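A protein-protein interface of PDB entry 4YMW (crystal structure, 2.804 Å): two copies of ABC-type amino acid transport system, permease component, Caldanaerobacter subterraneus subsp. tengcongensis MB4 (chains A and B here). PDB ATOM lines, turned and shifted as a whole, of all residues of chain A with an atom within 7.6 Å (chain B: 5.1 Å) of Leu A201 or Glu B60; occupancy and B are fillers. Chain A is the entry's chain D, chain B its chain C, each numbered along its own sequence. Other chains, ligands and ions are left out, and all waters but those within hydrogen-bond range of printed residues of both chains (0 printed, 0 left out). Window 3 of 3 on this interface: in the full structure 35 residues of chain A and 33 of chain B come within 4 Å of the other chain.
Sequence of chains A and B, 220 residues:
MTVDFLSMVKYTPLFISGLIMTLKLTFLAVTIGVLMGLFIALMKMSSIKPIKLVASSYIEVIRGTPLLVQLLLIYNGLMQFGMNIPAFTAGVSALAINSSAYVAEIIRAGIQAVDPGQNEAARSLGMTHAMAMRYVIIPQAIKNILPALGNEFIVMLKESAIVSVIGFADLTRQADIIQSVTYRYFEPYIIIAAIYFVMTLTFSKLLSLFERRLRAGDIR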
ATOM      1  N   ILE A 154      16.386  32.578   2.878  1.00  0.00           N
ATOM      2  CA  ILE A 154      15.550  31.733   2.032  1.00  0.00           C
ATOM      3  C   ILE A 154      15.184  30.428   2.734  1.00  0.00           C
ATOM      4  O   ILE A 154      14.042  29.988   2.660  1.00  0.00           O
ATOM      5  CB  ILE A 154      16.238  31.408   0.702  1.00  0.00           C
ATOM      6  CG1 ILE A 154      16.218  32.627  -0.208  1.00  0.00           C
ATOM      7  CG2 ILE A 154      15.558  30.239   0.003  1.00  0.00           C
ATOM      8  CD1 ILE A 154      16.829  32.348  -1.543  1.00  0.00           C
ATOM      9  N   LEU A 157      12.459  31.086   5.505  1.00  0.00           N
ATOM     10  CA  LEU A 157      11.084  31.102   5.007  1.00  0.00           C
ATOM     11  C   LEU A 157      10.411  29.744   5.150  1.00  0.00           C
ATOM     12  O   LEU A 157       9.369  29.623   5.794  1.00  0.00           O
ATOM     13  CB  LEU A 157      11.033  31.509   3.543  1.00  0.00           C
ATOM     14  CG  LEU A 157      11.018  32.999   3.240  1.00  0.00           C
ATOM     15  CD1 LEU A 157      10.841  33.170   1.735  1.00  0.00           C
ATOM     16  CD2 LEU A 157       9.934  33.718   4.027  1.00  0.00           C
ATOM     17  N   LYS A 158      11.012  28.724   4.556  1.00  0.00           N
ATOM     18  CA  LYS A 158      10.475  27.376   4.644  1.00  0.00           C
ATOM     19  C   LYS A 158      10.410  26.894   6.089  1.00  0.00           C
ATOM     20  O   LYS A 158       9.438  26.260   6.505  1.00  0.00           O
ATOM     21  CB  LYS A 158      11.313  26.396   3.819  1.00  0.00           C
ATOM     22  CG  LYS A 158      11.220  26.592   2.327  1.00  0.00           C
ATOM     23  CD  LYS A 158      11.815  25.395   1.598  1.00  0.00           C
ATOM     24  CE  LYS A 158      13.317  25.285   1.855  1.00  0.00           C
ATOM     25  NZ  LYS A 158      13.857  23.955   1.432  1.00  0.00           N
ATOM     26  N   ILE A 195       2.494  28.649  -3.141  1.00  0.00           N
ATOM     27  CA  ILE A 195       2.955  29.963  -2.676  1.00  0.00           C
ATOM     28  C   ILE A 195       4.394  29.895  -2.120  1.00  0.00           C
ATOM     29  O   ILE A 195       5.222  30.774  -2.413  1.00  0.00           O
ATOM     30  CB  ILE A 195       2.009  30.577  -1.594  1.00  0.00           C
ATOM     31  CG1 ILE A 195       0.646  30.917  -2.197  1.00  0.00           C
ATOM     32  CG2 ILE A 195       2.603  31.843  -0.995  1.00  0.00           C
ATOM     33  CD1 ILE A 195      -0.233  31.762  -1.297  1.00  0.00           C
ATOM     34  N   TYR A 196       4.693  28.863  -1.324  1.00  0.00           N
ATOM     35  CA  TYR A 196       6.054  28.689  -0.782  1.00  0.00           C
ATOM     36  C   TYR A 196       7.059  28.517  -1.917  1.00  0.00           C
ATOM     37  O   TYR A 196       8.154  29.090  -1.892  1.00  0.00           O
ATOM     38  CB  TYR A 196       6.145  27.487   0.176  1.00  0.00           C
ATOM     39  CG  TYR A 196       5.776  27.802   1.615  1.00  0.00           C
ATOM     40  CD1 TYR A 196       6.594  28.597   2.402  1.00  0.00           C
ATOM     41  CD2 TYR A 196       4.595  27.304   2.185  1.00  0.00           C
ATOM     42  CE1 TYR A 196       6.259  28.895   3.721  1.00  0.00           C
ATOM     43  CE2 TYR A 196       4.244  27.599   3.510  1.00  0.00           C
ATOM     44  CZ  TYR A 196       5.081  28.396   4.273  1.00  0.00           C
ATOM     45  OH  TYR A 196       4.752  28.695   5.580  1.00  0.00           O
ATOM     46  N   PHE A 197       6.663  27.736  -2.916  1.00  0.00           N
ATOM     47  CA  PHE A 197       7.495  27.472  -4.075  1.00  0.00           C
ATOM     48  C   PHE A 197       7.831  28.763  -4.794  1.00  0.00           C
ATOM     49  O   PHE A 197       9.003  29.056  -5.038  1.00  0.00           O
ATOM     50  CB  PHE A 197       6.792  26.508  -5.015  1.00  0.00           C
ATOM     51  CG  PHE A 197       7.607  26.123  -6.214  1.00  0.00           C
ATOM     52  CD1 PHE A 197       8.773  25.385  -6.063  1.00  0.00           C
ATOM     53  CD2 PHE A 197       7.179  26.446  -7.492  1.00  0.00           C
ATOM     54  CE1 PHE A 197       9.516  25.003  -7.166  1.00  0.00           C
ATOM     55  CE2 PHE A 197       7.910  26.062  -8.599  1.00  0.00           C
ATOM     56  CZ  PHE A 197       9.085  25.341  -8.437  1.00  0.00           C
ATOM     57  N   VAL A 198       6.803  29.537  -5.125  1.00  0.00           N
ATOM     58  CA  VAL A 198       7.024  30.804  -5.806  1.00  0.00           C
ATOM     59  C   VAL A 198       7.900  31.770  -4.985  1.00  0.00           C
ATOM     60  O   VAL A 198       8.807  32.411  -5.538  1.00  0.00           O
ATOM     61  CB  VAL A 198       5.687  31.462  -6.180  1.00  0.00           C
ATOM     62  CG1 VAL A 198       5.828  32.974  -6.266  1.00  0.00           C
ATOM     63  CG2 VAL A 198       5.190  30.885  -7.505  1.00  0.00           C
ATOM     64  N   MET A 199       7.680  31.853  -3.675  1.00  0.00           N
ATOM     65  CA  MET A 199       8.546  32.705  -2.846  1.00  0.00           C
ATOM     66  C   MET A 199      10.014  32.269  -2.911  1.00  0.00           C
ATOM     67  O   MET A 199      10.924  33.095  -3.107  1.00  0.00           O
ATOM     68  CB  MET A 199       8.100  32.696  -1.386  1.00  0.00           C
ATOM     69  CG  MET A 199       7.592  34.026  -0.870  1.00  0.00           C
ATOM     70  SD  MET A 199       7.355  33.921   0.911  1.00  0.00           S
ATOM     71  CE  MET A 199       6.415  32.391   1.015  1.00  0.00           C
ATOM     72  N   THR A 200      10.232  30.967  -2.739  1.00  0.00           N
ATOM     73  CA  THR A 200      11.567  30.391  -2.800  1.00  0.00           C
ATOM     74  C   THR A 200      12.252  30.678  -4.138  1.00  0.00           C
ATOM     75  O   THR A 200      13.408  31.084  -4.153  1.00  0.00           O
ATOM     76  CB  THR A 200      11.534  28.880  -2.527  1.00  0.00           C
ATOM     77  OG1 THR A 200      11.658  28.673  -1.112  1.00  0.00           O
ATOM     78  CG2 THR A 200      12.687  28.164  -3.241  1.00  0.00           C
ATOM     79  N   LEU A 201      11.544  30.496  -5.250  1.00  0.00           N
ATOM     80  CA  LEU A 201      12.107  30.832  -6.554  1.00  0.00           C
ATOM     81  C   LEU A 201      12.524  32.304  -6.608  1.00  0.00           C
ATOM     82  O   LEU A 201      13.688  32.632  -6.917  1.00  0.00           O
ATOM     83  CB  LEU A 201      11.109  30.552  -7.677  1.00  0.00           C
ATOM     84  CG  LEU A 201      10.849  29.131  -8.170  1.00  0.00           C
ATOM     85  CD1 LEU A 201      10.155  29.226  -9.506  1.00  0.00           C
ATOM     86  CD2 LEU A 201      12.104  28.275  -8.260  1.00  0.00           C
ATOM     87  N   THR A 202      11.579  33.184  -6.287  1.00  0.00           N
ATOM     88  CA  THR A 202      11.829  34.624  -6.336  1.00  0.00           C
ATOM     89  C   THR A 202      13.109  35.033  -5.594  1.00  0.00           C
ATOM     90  O   THR A 202      14.025  35.658  -6.170  1.00  0.00           O
ATOM     91  CB  THR A 202      10.629  35.407  -5.747  1.00  0.00           C
ATOM     92  OG1 THR A 202       9.499  35.256  -6.611  1.00  0.00           O
ATOM     93  CG2 THR A 202      10.950  36.886  -5.614  1.00  0.00           C
ATOM     94  N   PHE A 203      13.177  34.664  -4.319  1.00  0.00           N
ATOM     95  CA  PHE A 203      14.332  35.035  -3.517  1.00  0.00           C
ATOM     96  C   PHE A 203      15.613  34.326  -3.982  1.00  0.00           C
ATOM     97  O   PHE A 203      16.694  34.906  -3.894  1.00  0.00           O
ATOM     98  CB  PHE A 203      14.061  34.751  -2.042  1.00  0.00           C
ATOM     99  CG  PHE A 203      13.055  35.682  -1.429  1.00  0.00           C
ATOM    100  CD1 PHE A 203      13.265  37.047  -1.434  1.00  0.00           C
ATOM    101  CD2 PHE A 203      11.899  35.192  -0.845  1.00  0.00           C
ATOM    102  CE1 PHE A 203      12.338  37.904  -0.871  1.00  0.00           C
ATOM    103  CE2 PHE A 203      10.975  36.047  -0.281  1.00  0.00           C
ATOM    104  CZ  PHE A 203      11.194  37.402  -0.296  1.00  0.00           C
ATOM    105  N   SER A 204      15.489  33.105  -4.505  1.00  0.00           N
ATOM    106  CA  SER A 204      16.651  32.349  -4.982  1.00  0.00           C
ATOM    107  C   SER A 204      17.338  33.038  -6.149  1.00  0.00           C
ATOM    108  O   SER A 204      18.585  33.079  -6.237  1.00  0.00           O
ATOM    109  CB  SER A 204      16.257  30.933  -5.420  1.00  0.00           C
ATOM    110  OG  SER A 204      16.190  30.027  -4.330  1.00  0.00           O
ATOM    111  N   LYS A 205      16.536  33.605  -7.044  1.00  0.00           N
ATOM    112  CA  LYS A 205      17.155  34.256  -8.184  1.00  0.00           C
ATOM    113  C   LYS A 205      17.459  35.743  -7.969  1.00  0.00           C
ATOM    114  O   LYS A 205      18.338  36.285  -8.651  1.00  0.00           O
ATOM    115  CB  LYS A 205      16.319  34.025  -9.447  1.00  0.00           C
ATOM    116  CG  LYS A 205      16.523  32.591  -9.946  1.00  0.00           C
ATOM    117  CD  LYS A 205      16.242  32.387 -11.433  1.00  0.00           C
ATOM    118  CE  LYS A 205      14.875  32.881 -11.849  1.00  0.00           C
ATOM    119  NZ  LYS A 205      14.168  31.814 -12.617  1.00  0.00           N
ATOM    120  N   LEU A 206      16.834  36.409  -7.001  1.00  0.00           N
ATOM    121  CA  LEU A 206      17.356  37.748  -6.695  1.00  0.00           C
ATOM    122  C   LEU A 206      18.594  37.623  -5.813  1.00  0.00           C
ATOM    123  O   LEU A 206      19.391  38.578  -5.677  1.00  0.00           O
ATOM    124  CB  LEU A 206      16.311  38.645  -6.013  1.00  0.00           C
ATOM    125  CG  LEU A 206      14.961  38.831  -6.709  1.00  0.00           C
ATOM    126  CD1 LEU A 206      14.441  40.220  -6.368  1.00  0.00           C
ATOM    127  CD2 LEU A 206      15.061  38.631  -8.231  1.00  0.00           C
ATOM    128  N   LEU A 207      18.783  36.429  -5.255  1.00  0.00           N
ATOM    129  CA  LEU A 207      19.999  36.177  -4.524  1.00  0.00           C
ATOM    130  C   LEU A 207      21.096  35.798  -5.498  1.00  0.00           C
ATOM    131  O   LEU A 207      22.236  36.221  -5.315  1.00  0.00           O
ATOM    132  CB  LEU A 207      19.812  35.063  -3.498  1.00  0.00           C
ATOM    133  CG  LEU A 207      21.117  34.482  -2.960  1.00  0.00           C
ATOM    134  CD1 LEU A 207      21.755  35.498  -2.036  1.00  0.00           C
ATOM    135  CD2 LEU A 207      20.954  33.118  -2.283  1.00  0.00           C
ATOM    136  N   SER A 208      20.767  35.099  -6.583  1.00  0.00           N
ATOM    137  CA  SER A 208      21.836  34.788  -7.529  1.00  0.00           C
ATOM    138  C   SER A 208      22.232  36.038  -8.326  1.00  0.00           C
ATOM    139  O   SER A 208      23.424  36.266  -8.606  1.00  0.00           O
ATOM    140  CB  SER A 208      21.413  33.659  -8.471  1.00  0.00           C
ATOM    141  OG  SER A 208      20.329  34.046  -9.298  1.00  0.00           O
ATOM    142  N   ALA B  55      11.514  14.975 -13.536  1.00  0.00           N
ATOM    143  CA  ALA B  55      12.439  14.857 -12.412  1.00  0.00           C
ATOM    144  C   ALA B  55      12.932  16.205 -11.886  1.00  0.00           C
ATOM    145  O   ALA B  55      12.993  16.411 -10.673  1.00  0.00           O
ATOM    146  CB  ALA B  55      13.613  13.975 -12.793  1.00  0.00           C
ATOM    147  N   SER B  56      13.267  17.122 -12.791  1.00  0.00           N
ATOM    148  CA  SER B  56      13.832  18.407 -12.384  1.00  0.00           C
ATOM    149  C   SER B  56      12.808  19.313 -11.707  1.00  0.00           C
ATOM    150  O   SER B  56      13.136  20.065 -10.766  1.00  0.00           O
ATOM    151  CB  SER B  56      14.410  19.137 -13.602  1.00  0.00           C
ATOM    152  OG  SER B  56      15.436  18.390 -14.234  1.00  0.00           O
ATOM    153  N   SER B  57      11.549  19.180 -12.120  1.00  0.00           N
ATOM    154  CA  SER B  57      10.483  19.942 -11.469  1.00  0.00           C
ATOM    155  C   SER B  57      10.021  19.299 -10.169  1.00  0.00           C
ATOM    156  O   SER B  57       9.687  20.004  -9.224  1.00  0.00           O
ATOM    157  CB  SER B  57       9.310  20.108 -12.426  1.00  0.00           C
ATOM    158  OG  SER B  57       9.187  18.945 -13.222  1.00  0.00           O
ATOM    159  N   TYR B  58      10.040  17.966 -10.119  1.00  0.00           N
ATOM    160  CA  TYR B  58       9.850  17.233  -8.861  1.00  0.00           C
ATOM    161  C   TYR B  58      10.821  17.735  -7.798  1.00  0.00           C
ATOM    162  O   TYR B  58      10.407  18.251  -6.745  1.00  0.00           O
ATOM    163  CB  TYR B  58      10.044  15.736  -9.106  1.00  0.00           C
ATOM    164  CG  TYR B  58       9.992  14.806  -7.903  1.00  0.00           C
ATOM    165  CD1 TYR B  58       8.855  14.058  -7.626  1.00  0.00           C
ATOM    166  CD2 TYR B  58      11.110  14.612  -7.096  1.00  0.00           C
ATOM    167  CE1 TYR B  58       8.818  13.180  -6.560  1.00  0.00           C
ATOM    168  CE2 TYR B  58      11.084  13.730  -6.029  1.00  0.00           C
ATOM    169  CZ  TYR B  58       9.932  13.019  -5.766  1.00  0.00           C
ATOM    170  OH  TYR B  58       9.893  12.149  -4.700  1.00  0.00           O
ATOM    171  N   ILE B  59      12.113  17.601  -8.102  1.00  0.00           N
ATOM    172  CA  ILE B  59      13.197  18.029  -7.218  1.00  0.00           C
ATOM    173  C   ILE B  59      13.055  19.494  -6.813  1.00  0.00           C
ATOM    174  O   ILE B  59      13.123  19.837  -5.618  1.00  0.00           O
ATOM    175  CB  ILE B  59      14.568  17.811  -7.888  1.00  0.00           C
ATOM    176  CG1 ILE B  59      14.814  16.313  -8.105  1.00  0.00           C
ATOM    177  CG2 ILE B  59      15.684  18.424  -7.052  1.00  0.00           C
ATOM    178  CD1 ILE B  59      16.056  15.982  -8.903  1.00  0.00           C
ATOM    179  N   GLU B  60      12.849  20.357  -7.803  1.00  0.00           N
ATOM    180  CA  GLU B  60      12.788  21.785  -7.513  1.00  0.00           C
ATOM    181  C   GLU B  60      11.602  22.114  -6.615  1.00  0.00           C
ATOM    182  O   GLU B  60      11.703  22.982  -5.737  1.00  0.00           O
ATOM    183  CB  GLU B  60      12.722  22.608  -8.803  1.00  0.00           C
ATOM    184  CG  GLU B  60      13.382  23.980  -8.672  1.00  0.00           C
ATOM    185  CD  GLU B  60      13.541  24.693 -10.005  1.00  0.00           C
ATOM    186  OE1 GLU B  60      13.075  24.149 -11.038  1.00  0.00           O
ATOM    187  OE2 GLU B  60      14.140  25.794 -10.013  1.00  0.00           O
ATOM    188  N   VAL B  61      10.488  21.406  -6.827  1.00  0.00           N
ATOM    189  CA  VAL B  61       9.264  21.611  -6.043  1.00  0.00           C
ATOM    190  C   VAL B  61       9.453  21.184  -4.590  1.00  0.00           C
ATOM    191  O   VAL B  61       9.259  21.989  -3.676  1.00  0.00           O
ATOM    192  CB  VAL B  61       8.054  20.840  -6.662  1.00  0.00           C
ATOM    193  CG1 VAL B  61       6.983  20.545  -5.621  1.00  0.00           C
ATOM    194  CG2 VAL B  61       7.459  21.630  -7.815  1.00  0.00           C
ATOM    195  N   ILE B  62       9.902  19.948  -4.386  1.00  0.00           N
ATOM    196  CA  ILE B  62      10.113  19.445  -3.038  1.00  0.00           C
ATOM    197  C   ILE B  62      11.151  20.229  -2.238  1.00  0.00           C
ATOM    198  O   ILE B  62      10.945  20.494  -1.060  1.00  0.00           O
ATOM    199  CB  ILE B  62      10.532  17.976  -3.070  1.00  0.00           C
ATOM    200  CG1 ILE B  62       9.391  17.136  -3.624  1.00  0.00           C
ATOM    201  CG2 ILE B  62      10.961  17.485  -1.681  1.00  0.00           C
ATOM    202  CD1 ILE B  62       9.746  15.709  -3.748  1.00  0.00           C
ATOM    203  N   ARG B  63      12.257  20.642  -2.848  1.00  0.00           N
ATOM    204  CA  ARG B  63      13.261  21.303  -2.013  1.00  0.00           C
ATOM    205  C   ARG B  63      12.880  22.747  -1.729  1.00  0.00           C
ATOM    206  O   ARG B  63      13.347  23.331  -0.756  1.00  0.00           O
ATOM    207  CB  ARG B  63      14.656  21.245  -2.643  1.00  0.00           C
ATOM    208  CG  ARG B  63      15.091  19.868  -3.128  1.00  0.00           C
ATOM    209  CD  ARG B  63      16.585  19.868  -3.463  1.00  0.00           C
ATOM    210  NE  ARG B  63      17.145  21.217  -3.548  1.00  0.00           N
ATOM    211  CZ  ARG B  63      18.432  21.500  -3.378  1.00  0.00           C
ATOM    212  NH1 ARG B  63      19.287  20.525  -3.095  1.00  0.00           N
ATOM    213  NH2 ARG B  63      18.862  22.755  -3.469  1.00  0.00           N
ATOM    214  N   GLY B  64      12.035  23.318  -2.583  1.00  0.00           N
ATOM    215  CA  GLY B  64      11.646  24.706  -2.439  1.00  0.00           C
ATOM    216  C   GLY B  64      10.384  24.861  -1.618  1.00  0.00           C
ATOM    217  O   GLY B  64       9.790  25.943  -1.564  1.00  0.00           O
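Gly B64 touches Lys A158.
O of Tyr A196 touches O of Gly B64, at 3.6 Å.
O of Glu B60 touches CE1 of Phe A197, at 3.3 Å.
CA of Val B61 touches CE1 of Phe A197, at 3.6 Å.
Gly B64 touches Phe A197.
Glu B60 touches Leu A201 (OE2 to CD2, 3.7 Å).
Leu A201 touches just one residue of chain B: Glu B60.
Printed residues of chain A within 4 Å of Glu B60: Phe A197 and Leu A201.
Of the printed residues of chain B, Tyr A196 touches Gly B64.
Printed residues of chain B within 4 Å of Phe A197: Glu B60 (3.3 Å), Val B61 (3.6 Å) and Gly B64 (3.7 Å).
Printed residues of chain A within 4 Å of Arg B63: Lys A158 (2.3 Å).
Of the printed residues of chain B, Lys A158 touches Arg B63 and Gly B64.
Of the printed residues of chain A, Gly B64 touches Lys A158 (3.6 Å), Tyr A196 (3.6 Å), Phe A197 (3.7 Å) and Thr A200 (3.3 Å).
Ile B59 touches none of the printed residues of chain A.
Ser B56 touches none of the printed residues of chain A.
The nearest printed residue of chain B that does not touch Leu A201 is Gly B64 (6.1 Å).
The nearest printed residue of chain A that does not touch Val B61 is Lys A158 (6.8 Å).
Of the 17 printed residues of chain A, 5 touch a printed residue of chain B.
Along chain A the printed residues that touch a printed residue of chain B span positions 158 to 201.
Of the 10 printed residues of chain B, 4 touch a printed residue of chain A.
Printed residues of chain B that touch a printed residue of chain A: Glu B60, Val B61, Arg B63 and Gly B64.
Among the printed residues, no Asp or Glu carboxylate lies within 4 Å of a Lys or Arg side-chain nitrogen of the other chain.
The backbone carbonyl oxygen of Thr A200 is in hydrogen-bond range of the side-chain hydroxyl of Ser A204 (3.0 Å).
The backbone carbonyl oxygen (O) of Arg B63 lies close to the side-chain amino group (NZ) of Lys A158, 2.3 Å away.
The side-chain hydroxyl (OG1) of Thr A200 is in hydrogen-bond range of the backbone carbonyl oxygen (O) of Gly B64 (3.3 Å).
No position is printed for both chains.
Of the 8 pairs that touch across the chains among the printed residues, none has its exchanged pair printed and touching as well.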
